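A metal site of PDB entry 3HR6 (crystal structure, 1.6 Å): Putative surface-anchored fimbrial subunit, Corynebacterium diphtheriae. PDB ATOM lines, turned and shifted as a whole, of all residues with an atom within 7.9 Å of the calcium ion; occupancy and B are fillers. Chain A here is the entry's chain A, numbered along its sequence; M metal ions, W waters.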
ATOM      1  N   VAL A 152     -21.707 -29.635 -15.114  1.00  0.00           N
ATOM      2  CA  VAL A 152     -20.544 -28.856 -15.493  1.00  0.00           C
ATOM      3  C   VAL A 152     -21.058 -27.450 -15.836  1.00  0.00           C
ATOM      4  O   VAL A 152     -22.134 -27.308 -16.381  1.00  0.00           O
ATOM      5  CB  VAL A 152     -19.890 -29.501 -16.720  1.00  0.00           C
ATOM      6  CG1 VAL A 152     -18.825 -28.621 -17.295  1.00  0.00           C
ATOM      7  CG2 VAL A 152     -19.321 -30.886 -16.294  1.00  0.00           C
ATOM      8  N   ASP A 153     -20.307 -26.413 -15.481  1.00  0.00           N
ATOM      9  CA  ASP A 153     -20.612 -25.061 -15.937  1.00  0.00           C
ATOM     10  C   ASP A 153     -19.999 -24.924 -17.350  1.00  0.00           C
ATOM     11  O   ASP A 153     -18.754 -24.961 -17.530  1.00  0.00           O
ATOM     12  CB  ASP A 153     -19.995 -24.006 -15.021  1.00  0.00           C
ATOM     13  CG  ASP A 153     -20.337 -22.603 -15.444  1.00  0.00           C
ATOM     14  OD1 ASP A 153     -21.141 -22.446 -16.393  1.00  0.00           O
ATOM     15  OD2 ASP A 153     -19.815 -21.662 -14.792  1.00  0.00           O
ATOM     16  N   PRO A 154     -20.848 -24.782 -18.377  1.00  0.00           N
ATOM     17  CA  PRO A 154     -20.304 -24.752 -19.748  1.00  0.00           C
ATOM     18  C   PRO A 154     -19.712 -23.421 -20.169  1.00  0.00           C
ATOM     19  O   PRO A 154     -19.105 -23.319 -21.266  1.00  0.00           O
ATOM     20  CB  PRO A 154     -21.548 -25.046 -20.608  1.00  0.00           C
ATOM     21  CG  PRO A 154     -22.643 -24.583 -19.827  1.00  0.00           C
ATOM     22  CD  PRO A 154     -22.304 -24.809 -18.390  1.00  0.00           C
ATOM     23  N   ASP A 155     -19.921 -22.392 -19.359  1.00  0.00           N
ATOM     24  CA  ASP A 155     -19.420 -21.062 -19.658  1.00  0.00           C
ATOM     25  C   ASP A 155     -18.965 -20.429 -18.344  1.00  0.00           C
ATOM     26  O   ASP A 155     -19.769 -20.212 -17.458  1.00  0.00           O
ATOM     27  CB  ASP A 155     -20.523 -20.281 -20.323  1.00  0.00           C
ATOM     28  CG  ASP A 155     -20.071 -18.938 -20.806  1.00  0.00           C
ATOM     29  OD1 ASP A 155     -19.885 -18.055 -19.982  1.00  0.00           O
ATOM     30  OD2 ASP A 155     -19.925 -18.781 -22.022  1.00  0.00           O
ATOM     31  N   ALA A 156     -17.668 -20.128 -18.293  1.00  0.00           N
ATOM     32  CA  ALA A 156     -16.997 -19.592 -17.107  1.00  0.00           C
ATOM     33  C   ALA A 156     -17.120 -18.074 -16.955  1.00  0.00           C
ATOM     34  O   ALA A 156     -16.605 -17.543 -16.007  1.00  0.00           O
ATOM     35  CB  ALA A 156     -15.486 -19.985 -17.138  1.00  0.00           C
ATOM     36  N   THR A 157     -17.781 -17.387 -17.880  1.00  0.00           N
ATOM     37  CA  THR A 157     -17.924 -15.944 -17.776  1.00  0.00           C
ATOM     38  C   THR A 157     -18.553 -15.551 -16.456  1.00  0.00           C
ATOM     39  O   THR A 157     -18.149 -14.585 -15.833  1.00  0.00           O
ATOM     40  CB  THR A 157     -18.733 -15.412 -18.909  1.00  0.00           C
ATOM     41  OG1 THR A 157     -18.075 -15.818 -20.135  1.00  0.00           O
ATOM     42  CG2 THR A 157     -18.740 -13.891 -18.856  1.00  0.00           C
ATOM     43  N   GLN A 158     -19.549 -16.296 -16.039  1.00  0.00           N
ATOM     44  CA  GLN A 158     -20.097 -16.147 -14.687  1.00  0.00           C
ATOM     45  C   GLN A 158     -20.094 -17.498 -13.981  1.00  0.00           C
ATOM     46  O   GLN A 158     -20.543 -18.485 -14.535  1.00  0.00           O
ATOM     47  CB  GLN A 158     -21.510 -15.580 -14.735  1.00  0.00           C
ATOM     48  CG  GLN A 158     -22.158 -15.436 -13.333  1.00  0.00           C
ATOM     49  CD  GLN A 158     -23.442 -14.614 -13.384  1.00  0.00           C
ATOM     50  OE1 GLN A 158     -23.386 -13.383 -13.529  1.00  0.00           O
ATOM     51  NE2 GLN A 158     -24.588 -15.283 -13.210  1.00  0.00           N
ATOM     52  N   PRO A 159     -19.638 -17.538 -12.737  1.00  0.00           N
ATOM     53  CA  PRO A 159     -19.643 -18.853 -12.083  1.00  0.00           C
ATOM     54  C   PRO A 159     -21.006 -19.505 -12.023  1.00  0.00           C
ATOM     55  O   PRO A 159     -22.014 -18.853 -11.768  1.00  0.00           O
ATOM     56  CB  PRO A 159     -19.175 -18.521 -10.667  1.00  0.00           C
ATOM     57  CG  PRO A 159     -18.323 -17.327 -10.884  1.00  0.00           C
ATOM     58  CD  PRO A 159     -18.907 -16.528 -11.973  1.00  0.00           C
ATOM     59  N   GLY A 160     -21.018 -20.827 -12.184  1.00  0.00           N
ATOM     60  CA  GLY A 160     -22.240 -21.565 -12.065  1.00  0.00           C
ATOM     61  C   GLY A 160     -23.184 -21.419 -13.219  1.00  0.00           C
ATOM     62  O   GLY A 160     -22.815 -20.884 -14.322  1.00  0.00           O
ATOM     63  N   PHE A 161     -24.432 -21.823 -12.965  1.00  0.00           N
ATOM     64  CA  PHE A 161     -25.493 -21.767 -13.957  1.00  0.00           C
ATOM     65  C   PHE A 161     -26.738 -21.234 -13.294  1.00  0.00           C
ATOM     66  O   PHE A 161     -27.776 -21.889 -13.178  1.00  0.00           O
ATOM     67  CB  PHE A 161     -25.739 -23.095 -14.690  1.00  0.00           C
ATOM     68  CG  PHE A 161     -25.453 -24.326 -13.871  1.00  0.00           C
ATOM     69  CD1 PHE A 161     -26.447 -24.914 -13.084  1.00  0.00           C
ATOM     70  CD2 PHE A 161     -24.210 -24.942 -13.929  1.00  0.00           C
ATOM     71  CE1 PHE A 161     -26.173 -26.052 -12.361  1.00  0.00           C
ATOM     72  CE2 PHE A 161     -23.972 -26.090 -13.211  1.00  0.00           C
ATOM     73  CZ  PHE A 161     -24.952 -26.611 -12.389  1.00  0.00           C
ATOM     74  N   SER A 162     -26.647 -19.980 -12.860  1.00  0.00           N
ATOM     75  CA  SER A 162     -27.808 -19.277 -12.339  1.00  0.00           C
ATOM     76  C   SER A 162     -28.865 -19.152 -13.471  1.00  0.00           C
ATOM     77  O   SER A 162     -28.571 -19.298 -14.682  1.00  0.00           O
ATOM     78  CB  SER A 162     -27.368 -17.907 -11.871  1.00  0.00           C
ATOM     79  OG  SER A 162     -26.679 -17.931 -10.634  1.00  0.00           O
ATOM     80  N   GLU A 165     -28.526 -18.618 -17.557  1.00  0.00           N
ATOM     81  CA  GLU A 165     -27.387 -19.289 -18.171  1.00  0.00           C
ATOM     82  C   GLU A 165     -27.731 -20.769 -18.466  1.00  0.00           C
ATOM     83  O   GLU A 165     -28.774 -21.279 -18.107  1.00  0.00           O
ATOM     84  CB  GLU A 165     -26.206 -19.254 -17.194  1.00  0.00           C
ATOM     85  CG  GLU A 165     -25.702 -17.832 -16.880  1.00  0.00           C
ATOM     86  CD  GLU A 165     -24.184 -17.776 -16.769  1.00  0.00           C
ATOM     87  OE1 GLU A 165     -23.587 -18.550 -16.016  1.00  0.00           O
ATOM     88  OE2 GLU A 165     -23.586 -16.923 -17.435  1.00  0.00           O
ATOM     89  N   ASN A 166     -26.790 -21.433 -19.126  1.00  0.00           N
ATOM     90  CA  ASN A 166     -26.927 -22.839 -19.389  1.00  0.00           C
ATOM     91  C   ASN A 166     -26.168 -23.714 -18.406  1.00  0.00           C
ATOM     92  O   ASN A 166     -25.098 -23.381 -17.921  1.00  0.00           O
ATOM     93  CB  ASN A 166     -26.433 -23.158 -20.786  1.00  0.00           C
ATOM     94  CG  ASN A 166     -27.170 -22.389 -21.848  1.00  0.00           C
ATOM     95  OD1 ASN A 166     -28.389 -22.389 -21.911  1.00  0.00           O
ATOM     96  ND2 ASN A 166     -26.409 -21.690 -22.686  1.00  0.00           N
ATOM     97  N   VAL A 167     -26.781 -24.865 -18.126  1.00  0.00           N
ATOM     98  CA  VAL A 167     -26.159 -25.958 -17.408  1.00  0.00           C
ATOM     99  C   VAL A 167     -25.709 -26.971 -18.433  1.00  0.00           C
ATOM    100  O   VAL A 167     -26.280 -27.062 -19.520  1.00  0.00           O
ATOM    101  CB  VAL A 167     -27.116 -26.581 -16.362  1.00  0.00           C
ATOM    102  CG1 VAL A 167     -28.454 -27.171 -17.005  1.00  0.00           C
ATOM    103  CG2 VAL A 167     -26.381 -27.642 -15.464  1.00  0.00           C
ATOM    104  N   HIS A 368     -27.553 -19.705  -8.566  1.00  0.00           N
ATOM    105  CA  HIS A 368     -27.025 -21.074  -8.423  1.00  0.00           C
ATOM    106  C   HIS A 368     -25.829 -21.009  -7.498  1.00  0.00           C
ATOM    107  O   HIS A 368     -24.821 -20.357  -7.775  1.00  0.00           O
ATOM    108  CB  HIS A 368     -26.641 -21.644  -9.784  1.00  0.00           C
ATOM    109  CG  HIS A 368     -25.849 -22.909  -9.696  1.00  0.00           C
ATOM    110  ND1 HIS A 368     -24.720 -23.173 -10.467  1.00  0.00           N
ATOM    111  CD2 HIS A 368     -26.010 -23.999  -8.906  1.00  0.00           C
ATOM    112  CE1 HIS A 368     -24.255 -24.365 -10.170  1.00  0.00           C
ATOM    113  NE2 HIS A 368     -24.995 -24.870  -9.193  1.00  0.00           N
HETATM  114 CA    CA M   1     -21.528 -20.060 -16.053  1.00  0.00          CA
HETATM  115  O   HOH W   1     -23.127 -20.980 -17.927  1.00  0.00           O
HETATM  116  O   HOH W   2     -21.249 -17.945 -17.568  1.00  0.00           O
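OG1 of Thr 157 sits at hydrogen-bond distance from OD1 of Asp 155 (2.9 Å).
Five residues have an atom within 4 Å of the calcium ion: Asp 153, Asp 155, Gln 158, Gly 160 and Glu 165. The nearest printed residue that does not touch the calcium ion is Pro 159 (4.1 Å).
The calcium ion is bound by O of Asp 155 (2.3 Å), O of Gly 160 (2.3 Å), O of Gln 158 (2.4 Å), OD1 of Asp 153 (2.4 Å), OE1 of Glu 165 (2.6 Å), water W2 (2.6 Å), water W1 (2.6 Å) and OD2 of Asp 153 (2.7 Å). The calcium ion has eight donor atoms within binding distance.
Water W2 lies within hydrogen-bond range of OE2 of Glu 165, OD1 of Asp 155 and N of Gln 158.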
